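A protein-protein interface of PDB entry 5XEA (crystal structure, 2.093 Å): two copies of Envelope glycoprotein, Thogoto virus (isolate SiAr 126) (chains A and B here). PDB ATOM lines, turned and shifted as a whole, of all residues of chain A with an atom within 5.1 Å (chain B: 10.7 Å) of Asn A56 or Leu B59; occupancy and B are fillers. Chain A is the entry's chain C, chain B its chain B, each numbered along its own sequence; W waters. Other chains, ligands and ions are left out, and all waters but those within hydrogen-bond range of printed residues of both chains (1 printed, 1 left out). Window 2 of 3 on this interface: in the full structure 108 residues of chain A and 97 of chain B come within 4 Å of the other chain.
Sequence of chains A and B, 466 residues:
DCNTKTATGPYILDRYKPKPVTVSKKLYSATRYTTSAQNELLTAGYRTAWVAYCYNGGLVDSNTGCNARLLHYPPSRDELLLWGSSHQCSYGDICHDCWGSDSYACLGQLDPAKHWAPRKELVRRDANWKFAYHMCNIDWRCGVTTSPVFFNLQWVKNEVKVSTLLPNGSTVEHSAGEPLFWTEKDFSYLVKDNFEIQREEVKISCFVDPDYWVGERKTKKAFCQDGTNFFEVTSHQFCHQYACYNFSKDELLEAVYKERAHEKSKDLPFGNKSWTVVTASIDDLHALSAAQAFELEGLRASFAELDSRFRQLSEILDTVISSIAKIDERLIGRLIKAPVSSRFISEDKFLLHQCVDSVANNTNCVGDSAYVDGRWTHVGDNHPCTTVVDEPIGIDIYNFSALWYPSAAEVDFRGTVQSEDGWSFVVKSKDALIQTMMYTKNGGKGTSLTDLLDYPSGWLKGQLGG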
ATOM      1  N   CYS A  54     -26.232  23.060 -36.468  1.00  0.00           N
ATOM      2  CA  CYS A  54     -25.143  22.629 -35.605  1.00  0.00           C
ATOM      3  C   CYS A  54     -25.625  21.553 -34.643  1.00  0.00           C
ATOM      4  O   CYS A  54     -26.812  21.483 -34.312  1.00  0.00           O
ATOM      5  CB  CYS A  54     -24.590  23.808 -34.808  1.00  0.00           C
ATOM      6  SG  CYS A  54     -24.179  25.248 -35.874  1.00  0.00           S
ATOM      7  N   TYR A  55     -24.690  20.714 -34.202  1.00  0.00           N
ATOM      8  CA  TYR A  55     -24.932  19.743 -33.138  1.00  0.00           C
ATOM      9  C   TYR A  55     -23.864  19.931 -32.087  1.00  0.00           C
ATOM     10  O   TYR A  55     -22.683  20.070 -32.423  1.00  0.00           O
ATOM     11  CB  TYR A  55     -24.910  18.303 -33.637  1.00  0.00           C
ATOM     12  CG  TYR A  55     -25.119  17.306 -32.498  1.00  0.00           C
ATOM     13  CD1 TYR A  55     -26.340  17.228 -31.845  1.00  0.00           C
ATOM     14  CD2 TYR A  55     -24.090  16.477 -32.058  1.00  0.00           C
ATOM     15  CE1 TYR A  55     -26.550  16.366 -30.800  1.00  0.00           C
ATOM     16  CE2 TYR A  55     -24.295  15.575 -30.992  1.00  0.00           C
ATOM     17  CZ  TYR A  55     -25.532  15.534 -30.371  1.00  0.00           C
ATOM     18  OH  TYR A  55     -25.770  14.662 -29.321  1.00  0.00           O
ATOM     19  N   ASN A  56     -24.293  19.993 -30.826  1.00  0.00           N
ATOM     20  CA  ASN A  56     -23.401  20.137 -29.682  1.00  0.00           C
ATOM     21  C   ASN A  56     -23.528  18.867 -28.844  1.00  0.00           C
ATOM     22  O   ASN A  56     -24.493  18.713 -28.087  1.00  0.00           O
ATOM     23  CB  ASN A  56     -23.735  21.387 -28.865  1.00  0.00           C
ATOM     24  CG  ASN A  56     -22.843  21.535 -27.633  1.00  0.00           C
ATOM     25  OD1 ASN A  56     -21.972  20.700 -27.380  1.00  0.00           O
ATOM     26  ND2 ASN A  56     -23.041  22.612 -26.877  1.00  0.00           N
ATOM     27  N   GLY A  57     -22.549  17.969 -28.978  1.00  0.00           N
ATOM     28  CA  GLY A  57     -22.461  16.808 -28.111  1.00  0.00           C
ATOM     29  C   GLY A  57     -21.126  16.759 -27.399  1.00  0.00           C
ATOM     30  O   GLY A  57     -20.677  15.696 -26.979  1.00  0.00           O
ATOM     31  N   GLY A  58     -20.481  17.912 -27.246  1.00  0.00           N
ATOM     32  CA  GLY A  58     -19.168  17.968 -26.640  1.00  0.00           C
ATOM     33  C   GLY A  58     -18.086  17.582 -27.631  1.00  0.00           C
ATOM     34  O   GLY A  58     -18.335  16.936 -28.636  1.00  0.00           O
ATOM     35  N   LEU A  59     -16.858  18.017 -27.343  1.00  0.00           N
ATOM     36  CA  LEU A  59     -15.750  17.827 -28.271  1.00  0.00           C
ATOM     37  C   LEU A  59     -15.346  16.369 -28.433  1.00  0.00           C
ATOM     38  O   LEU A  59     -14.652  16.043 -29.407  1.00  0.00           O
ATOM     39  CB  LEU A  59     -14.540  18.648 -27.829  1.00  0.00           C
ATOM     40  CG  LEU A  59     -14.652  20.125 -28.246  1.00  0.00           C
ATOM     41  CD1 LEU A  59     -13.355  20.880 -27.991  1.00  0.00           C
ATOM     42  CD2 LEU A  59     -15.087  20.245 -29.714  1.00  0.00           C
ATOM     43  N   THR A  64     -20.063  16.611 -33.316  1.00  0.00           N
ATOM     44  CA  THR A  64     -20.190  17.986 -32.879  1.00  0.00           C
ATOM     45  C   THR A  64     -19.626  18.912 -33.948  1.00  0.00           C
ATOM     46  O   THR A  64     -18.519  18.699 -34.455  1.00  0.00           O
ATOM     47  CB  THR A  64     -19.457  18.192 -31.567  1.00  0.00           C
ATOM     48  OG1 THR A  64     -20.116  17.436 -30.541  1.00  0.00           O
ATOM     49  CG2 THR A  64     -19.443  19.682 -31.179  1.00  0.00           C
ATOM     50  N   ASN A 128     -24.297  27.360 -30.999  1.00  0.00           N
ATOM     51  CA  ASN A 128     -24.404  25.921 -30.783  1.00  0.00           C
ATOM     52  C   ASN A 128     -24.311  25.639 -29.283  1.00  0.00           C
ATOM     53  O   ASN A 128     -23.559  24.779 -28.838  1.00  0.00           O
ATOM     54  CB  ASN A 128     -23.302  25.197 -31.562  1.00  0.00           C
ATOM     55  CG  ASN A 128     -23.472  23.676 -31.582  1.00  0.00           C
ATOM     56  OD1 ASN A 128     -24.573  23.146 -31.409  1.00  0.00           O
ATOM     57  ND2 ASN A 128     -22.374  22.974 -31.847  1.00  0.00           N
ATOM     58  N   TRP A 129     -25.071  26.376 -28.478  1.00  0.00           N
ATOM     59  CA  TRP A 129     -24.839  26.439 -27.040  1.00  0.00           C
ATOM     60  C   TRP A 129     -25.666  25.441 -26.229  1.00  0.00           C
ATOM     61  O   TRP A 129     -25.554  25.427 -24.997  1.00  0.00           O
ATOM     62  CB  TRP A 129     -25.103  27.857 -26.518  1.00  0.00           C
ATOM     63  CG  TRP A 129     -26.412  28.493 -26.924  1.00  0.00           C
ATOM     64  CD1 TRP A 129     -26.598  29.477 -27.877  1.00  0.00           C
ATOM     65  CD2 TRP A 129     -27.705  28.237 -26.362  1.00  0.00           C
ATOM     66  NE1 TRP A 129     -27.926  29.822 -27.939  1.00  0.00           N
ATOM     67  CE2 TRP A 129     -28.623  29.071 -27.020  1.00  0.00           C
ATOM     68  CE3 TRP A 129     -28.180  27.362 -25.375  1.00  0.00           C
ATOM     69  CZ2 TRP A 129     -29.989  29.060 -26.719  1.00  0.00           C
ATOM     70  CZ3 TRP A 129     -29.527  27.359 -25.080  1.00  0.00           C
ATOM     71  CH2 TRP A 129     -30.413  28.205 -25.752  1.00  0.00           C
ATOM     72  N   LYS A 130     -26.473  24.607 -26.873  1.00  0.00           N
ATOM     73  CA  LYS A 130     -27.425  23.727 -26.189  1.00  0.00           C
ATOM     74  C   LYS A 130     -26.922  22.290 -26.256  1.00  0.00           C
ATOM     75  O   LYS A 130     -27.126  21.599 -27.256  1.00  0.00           O
ATOM     76  CB  LYS A 130     -28.805  23.874 -26.821  1.00  0.00           C
ATOM     77  CG  LYS A 130     -29.896  23.112 -26.130  1.00  0.00           C
ATOM     78  CD  LYS A 130     -30.623  23.952 -25.116  1.00  0.00           C
ATOM     79  CE  LYS A 130     -31.544  23.086 -24.263  1.00  0.00           C
ATOM     80  NZ  LYS A 130     -32.329  23.915 -23.309  1.00  0.00           N
ATOM     81  N   PHE A 131     -26.310  21.833 -25.163  1.00  0.00           N
ATOM     82  CA  PHE A 131     -25.671  20.522 -25.125  1.00  0.00           C
ATOM     83  C   PHE A 131     -26.682  19.388 -25.285  1.00  0.00           C
ATOM     84  O   PHE A 131     -27.767  19.413 -24.703  1.00  0.00           O
ATOM     85  CB  PHE A 131     -24.910  20.351 -23.811  1.00  0.00           C
ATOM     86  CG  PHE A 131     -24.200  19.028 -23.683  1.00  0.00           C
ATOM     87  CD1 PHE A 131     -22.968  18.827 -24.287  1.00  0.00           C
ATOM     88  CD2 PHE A 131     -24.747  17.991 -22.923  1.00  0.00           C
ATOM     89  CE1 PHE A 131     -22.301  17.615 -24.164  1.00  0.00           C
ATOM     90  CE2 PHE A 131     -24.090  16.772 -22.802  1.00  0.00           C
ATOM     91  CZ  PHE A 131     -22.864  16.583 -23.421  1.00  0.00           C
ATOM     92  N   ALA A 132     -26.294  18.384 -26.075  1.00  0.00           N
ATOM     93  CA  ALA A 132     -27.095  17.222 -26.467  1.00  0.00           C
ATOM     94  C   ALA A 132     -28.196  17.576 -27.463  1.00  0.00           C
ATOM     95  O   ALA A 132     -29.076  16.754 -27.717  1.00  0.00           O
ATOM     96  CB  ALA A 132     -27.689  16.473 -25.245  1.00  0.00           C
ATOM     97  N   TYR A 133     -28.142  18.760 -28.087  1.00  0.00           N
ATOM     98  CA  TYR A 133     -29.189  19.197 -28.999  1.00  0.00           C
ATOM     99  C   TYR A 133     -28.599  19.758 -30.292  1.00  0.00           C
ATOM    100  O   TYR A 133     -27.446  20.213 -30.348  1.00  0.00           O
ATOM    101  CB  TYR A 133     -30.101  20.261 -28.352  1.00  0.00           C
ATOM    102  CG  TYR A 133     -31.026  19.707 -27.284  1.00  0.00           C
ATOM    103  CD1 TYR A 133     -32.312  19.274 -27.607  1.00  0.00           C
ATOM    104  CD2 TYR A 133     -30.610  19.603 -25.954  1.00  0.00           C
ATOM    105  CE1 TYR A 133     -33.164  18.751 -26.631  1.00  0.00           C
ATOM    106  CE2 TYR A 133     -31.457  19.072 -24.970  1.00  0.00           C
ATOM    107  CZ  TYR A 133     -32.728  18.655 -25.316  1.00  0.00           C
ATOM    108  OH  TYR A 133     -33.575  18.138 -24.356  1.00  0.00           O
ATOM    109  N   TYR B  55     -15.865  33.376 -22.866  1.00  0.00           N
ATOM    110  CA  TYR B  55     -15.832  32.547 -21.666  1.00  0.00           C
ATOM    111  C   TYR B  55     -15.758  31.086 -22.078  1.00  0.00           C
ATOM    112  O   TYR B  55     -16.485  30.646 -22.973  1.00  0.00           O
ATOM    113  CB  TYR B  55     -17.055  32.770 -20.753  1.00  0.00           C
ATOM    114  CG  TYR B  55     -17.062  31.848 -19.538  1.00  0.00           C
ATOM    115  CD1 TYR B  55     -16.157  32.034 -18.499  1.00  0.00           C
ATOM    116  CD2 TYR B  55     -17.955  30.776 -19.444  1.00  0.00           C
ATOM    117  CE1 TYR B  55     -16.153  31.194 -17.385  1.00  0.00           C
ATOM    118  CE2 TYR B  55     -17.955  29.927 -18.320  1.00  0.00           C
ATOM    119  CZ  TYR B  55     -17.045  30.151 -17.302  1.00  0.00           C
ATOM    120  OH  TYR B  55     -17.004  29.335 -16.196  1.00  0.00           O
ATOM    121  N   ASN B  56     -14.866  30.348 -21.436  1.00  0.00           N
ATOM    122  CA  ASN B  56     -14.690  28.925 -21.686  1.00  0.00           C
ATOM    123  C   ASN B  56     -15.203  28.155 -20.464  1.00  0.00           C
ATOM    124  O   ASN B  56     -14.497  28.029 -19.463  1.00  0.00           O
ATOM    125  CB  ASN B  56     -13.220  28.619 -21.949  1.00  0.00           C
ATOM    126  CG  ASN B  56     -12.981  27.172 -22.316  1.00  0.00           C
ATOM    127  OD1 ASN B  56     -13.866  26.331 -22.194  1.00  0.00           O
ATOM    128  ND2 ASN B  56     -11.777  26.879 -22.782  1.00  0.00           N
ATOM    129  N   GLY B  57     -16.418  27.622 -20.553  1.00  0.00           N
ATOM    130  CA  GLY B  57     -16.933  26.753 -19.492  1.00  0.00           C
ATOM    131  C   GLY B  57     -17.152  25.322 -19.952  1.00  0.00           C
ATOM    132  O   GLY B  57     -17.882  24.560 -19.313  1.00  0.00           O
ATOM    133  N   GLY B  58     -16.510  24.940 -21.068  1.00  0.00           N
ATOM    134  CA  GLY B  58     -16.741  23.654 -21.695  1.00  0.00           C
ATOM    135  C   GLY B  58     -18.038  23.691 -22.491  1.00  0.00           C
ATOM    136  O   GLY B  58     -18.865  24.577 -22.255  1.00  0.00           O
ATOM    137  N   LEU B  59     -18.255  22.759 -23.432  1.00  0.00           N
ATOM    138  CA  LEU B  59     -19.431  22.863 -24.294  1.00  0.00           C
ATOM    139  C   LEU B  59     -20.732  22.544 -23.562  1.00  0.00           C
ATOM    140  O   LEU B  59     -21.804  22.893 -24.056  1.00  0.00           O
ATOM    141  CB  LEU B  59     -19.279  21.959 -25.516  1.00  0.00           C
ATOM    142  CG  LEU B  59     -18.379  22.557 -26.622  1.00  0.00           C
ATOM    143  CD1 LEU B  59     -18.489  21.790 -27.945  1.00  0.00           C
ATOM    144  CD2 LEU B  59     -18.708  24.030 -26.815  1.00  0.00           C
ATOM    145  N   VAL B  60     -20.675  21.874 -22.403  1.00  0.00           N
ATOM    146  CA  VAL B  60     -21.909  21.601 -21.666  1.00  0.00           C
ATOM    147  C   VAL B  60     -22.517  22.897 -21.151  1.00  0.00           C
ATOM    148  O   VAL B  60     -23.739  23.019 -21.049  1.00  0.00           O
ATOM    149  CB  VAL B  60     -21.653  20.594 -20.521  1.00  0.00           C
ATOM    150  CG1 VAL B  60     -22.918  20.390 -19.686  1.00  0.00           C
ATOM    151  CG2 VAL B  60     -21.177  19.262 -21.077  1.00  0.00           C
ATOM    152  N   ASP B  61     -21.691  23.899 -20.863  1.00  0.00           N
ATOM    153  CA  ASP B  61     -22.154  25.174 -20.325  1.00  0.00           C
ATOM    154  C   ASP B  61     -22.615  26.099 -21.460  1.00  0.00           C
ATOM    155  O   ASP B  61     -21.828  26.431 -22.357  1.00  0.00           O
ATOM    156  CB  ASP B  61     -21.024  25.809 -19.519  1.00  0.00           C
ATOM    157  CG  ASP B  61     -21.448  27.064 -18.787  1.00  0.00           C
ATOM    158  OD1 ASP B  61     -22.439  27.721 -19.204  1.00  0.00           O
ATOM    159  OD2 ASP B  61     -20.773  27.403 -17.794  1.00  0.00           O
ATOM    160  N   SER B  62     -23.873  26.568 -21.379  1.00  0.00           N
ATOM    161  CA  SER B  62     -24.484  27.380 -22.426  1.00  0.00           C
ATOM    162  C   SER B  62     -23.937  28.806 -22.489  1.00  0.00           C
ATOM    163  O   SER B  62     -24.225  29.514 -23.458  1.00  0.00           O
ATOM    164  CB  SER B  62     -26.008  27.424 -22.246  1.00  0.00           C
ATOM    165  OG  SER B  62     -26.377  28.074 -21.035  1.00  0.00           O
ATOM    166  N   ASN B  63     -23.171  29.251 -21.498  1.00  0.00           N
ATOM    167  CA  ASN B  63     -22.479  30.527 -21.610  1.00  0.00           C
ATOM    168  C   ASN B  63     -21.095  30.398 -22.224  1.00  0.00           C
ATOM    169  O   ASN B  63     -20.361  31.382 -22.248  1.00  0.00           O
ATOM    170  CB  ASN B  63     -22.337  31.188 -20.243  1.00  0.00           C
ATOM    171  CG  ASN B  63     -23.637  31.249 -19.493  1.00  0.00           C
ATOM    172  OD1 ASN B  63     -23.789  30.615 -18.443  1.00  0.00           O
ATOM    173  ND2 ASN B  63     -24.584  32.009 -20.015  1.00  0.00           N
ATOM    174  N   THR B  64     -20.684  29.212 -22.666  1.00  0.00           N
ATOM    175  CA  THR B  64     -19.399  29.116 -23.353  1.00  0.00           C
ATOM    176  C   THR B  64     -19.550  29.743 -24.737  1.00  0.00           C
ATOM    177  O   THR B  64     -20.527  29.479 -25.444  1.00  0.00           O
ATOM    178  CB  THR B  64     -18.928  27.661 -23.454  1.00  0.00           C
ATOM    179  OG1 THR B  64     -18.568  27.159 -22.149  1.00  0.00           O
ATOM    180  CG2 THR B  64     -17.715  27.549 -24.381  1.00  0.00           C
ATOM    181  N   GLY B  65     -18.637  30.614 -25.105  1.00  0.00           N
ATOM    182  CA  GLY B  65     -18.766  31.302 -26.375  1.00  0.00           C
ATOM    183  C   GLY B  65     -18.079  32.648 -26.318  1.00  0.00           C
ATOM    184  O   GLY B  65     -17.374  32.954 -25.372  1.00  0.00           O
ATOM    185  N   CYS B  66     -18.292  33.450 -27.365  1.00  0.00           N
ATOM    186  CA  CYS B  66     -17.622  34.743 -27.491  1.00  0.00           C
ATOM    187  C   CYS B  66     -18.591  35.830 -27.918  1.00  0.00           C
ATOM    188  O   CYS B  66     -19.510  35.598 -28.715  1.00  0.00           O
ATOM    189  CB  CYS B  66     -16.478  34.724 -28.518  1.00  0.00           C
ATOM    190  SG  CYS B  66     -15.023  33.745 -28.085  1.00  0.00           S
ATOM    191  N   ASN B 128      -9.858  31.537 -26.586  1.00  0.00           N
ATOM    192  CA  ASN B 128     -10.698  31.183 -25.443  1.00  0.00           C
ATOM    193  C   ASN B 128     -10.156  29.897 -24.829  1.00  0.00           C
ATOM    194  O   ASN B 128     -10.915  28.950 -24.632  1.00  0.00           O
ATOM    195  CB  ASN B 128     -12.150  30.985 -25.909  1.00  0.00           C
ATOM    196  CG  ASN B 128     -13.170  30.965 -24.766  1.00  0.00           C
ATOM    197  OD1 ASN B 128     -12.914  31.446 -23.659  1.00  0.00           O
ATOM    198  ND2 ASN B 128     -14.361  30.441 -25.062  1.00  0.00           N
ATOM    199  N   PHE B 131      -9.704  27.286 -19.660  1.00  0.00           N
ATOM    200  CA  PHE B 131     -10.906  26.648 -19.141  1.00  0.00           C
ATOM    201  C   PHE B 131     -11.335  27.264 -17.817  1.00  0.00           C
ATOM    202  O   PHE B 131     -10.509  27.504 -16.934  1.00  0.00           O
ATOM    203  CB  PHE B 131     -10.685  25.149 -18.954  1.00  0.00           C
ATOM    204  CG  PHE B 131     -11.878  24.446 -18.366  1.00  0.00           C
ATOM    205  CD1 PHE B 131     -13.036  24.297 -19.105  1.00  0.00           C
ATOM    206  CD2 PHE B 131     -11.842  23.941 -17.053  1.00  0.00           C
ATOM    207  CE1 PHE B 131     -14.138  23.659 -18.573  1.00  0.00           C
ATOM    208  CE2 PHE B 131     -12.946  23.304 -16.509  1.00  0.00           C
ATOM    209  CZ  PHE B 131     -14.096  23.152 -17.268  1.00  0.00           C
ATOM    210  N   ALA B 132     -12.646  27.518 -17.702  1.00  0.00           N
ATOM    211  CA  ALA B 132     -13.308  28.087 -16.531  1.00  0.00           C
ATOM    212  C   ALA B 132     -12.904  29.518 -16.280  1.00  0.00           C
ATOM    213  O   ALA B 132     -13.056  30.016 -15.152  1.00  0.00           O
ATOM    214  CB  ALA B 132     -13.064  27.244 -15.257  1.00  0.00           C
HETATM  215  O   HOH W   1     -25.728  23.592 -23.016  1.00  0.00           O
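O of Leu B59 lies within hydrogen-bond range of ND2 of Asn A56 (3.1 Å).
Asn A56 touches Leu B59, but with the chains exchanged Leu A59 does not touch Asn B56 (8.0 Å).
Thr A64 touches Leu B59, but with the chains exchanged Leu A59 does not touch Thr B64 (8.7 Å).
Positions printed for both chains: 55, 56, 57, 58, 59, 64, 128, 131 and 132.
No residue of chain B comes within 4 Å of Tyr A55.
Asn A56 touches just one residue of chain B: Leu B59.
No residue of chain B comes within 4 Å of Gly A57.
Gly A58 touches none of the printed residues of chain B.
Of the printed residues of chain B, Thr A64 touches Leu B59 (3.98 Å).
No residue of chain B comes within 4 Å of Asn A128.
Printed residues of chain B within 4 Å of Trp A129: Ser B62 (3.4 Å).
No residue of chain B comes within 4 Å of Ala A132.
Leu B59 touches just these residues of chain A: Asn A56 and Thr A64.
Asp B61 touches none of the printed residues of chain A.
Asn B63 touches none of the printed residues of chain A.
The nearest residue of chain B that does not touch Asn A56 is Val B60 (5.1 Å).
The nearest residue of chain A that does not touch Leu B59 is Phe A131 (4.02 Å).
The nearest printed residue of chain A that does not touch Val B60 is Trp A129 (5.0 Å).
CD1 of Leu B59 touches CG2 of Thr A64, 3.98 Å away.
Ser B62 touches Trp A129 (CA to O, 3.4 Å).
CG2 of Val B60 touches CE1 of Phe A131, at 3.7 Å.
The side-chain amide oxygen of Asn A56 sits at hydrogen-bond distance from the backbone NH of Gly A58 (3.2 Å).
The side-chain amide nitrogen (ND2) of Asn A56 lies within hydrogen-bond range of the backbone carbonyl oxygen (O) of Asn A128.
N of Ala A132 lies within hydrogen-bond range of O of Asn A56, at 2.7 Å.
The backbone NH of Asn A56 sits at hydrogen-bond distance from the backbone carbonyl oxygen of Tyr A133 (3.2 Å).
The side-chain hydroxyl (OG1) of Thr A64 is in hydrogen-bond range of the backbone NH (N) of Gly A57 (2.9 Å).
O of Gly A58 sits at hydrogen-bond distance from OG1 of Thr A64.
Water W1 lies within hydrogen-bond range of the backbone carbonyl oxygen (O) of Trp A129 (2.7 Å), the backbone NH (N) of Phe A131 (2.8 Å) and the backbone carbonyl oxygen (O) of Val B60 (2.9 Å).
Printed residues of chain A that touch a printed residue of chain B: Asn A56, Thr A64, Trp A129 and Phe A131.
Hydrophobic or aromatic side chains of chain A that line the printed part of chain B: Trp A129 and Phe A131.
Hydrophobic or aromatic side chains of chain B that line the printed part of chain A: Leu B59 and Val B60.
Among the printed residues, no Asp or Glu carboxylate lies within 4 Å of a Lys or Arg side-chain nitrogen of the other chain.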
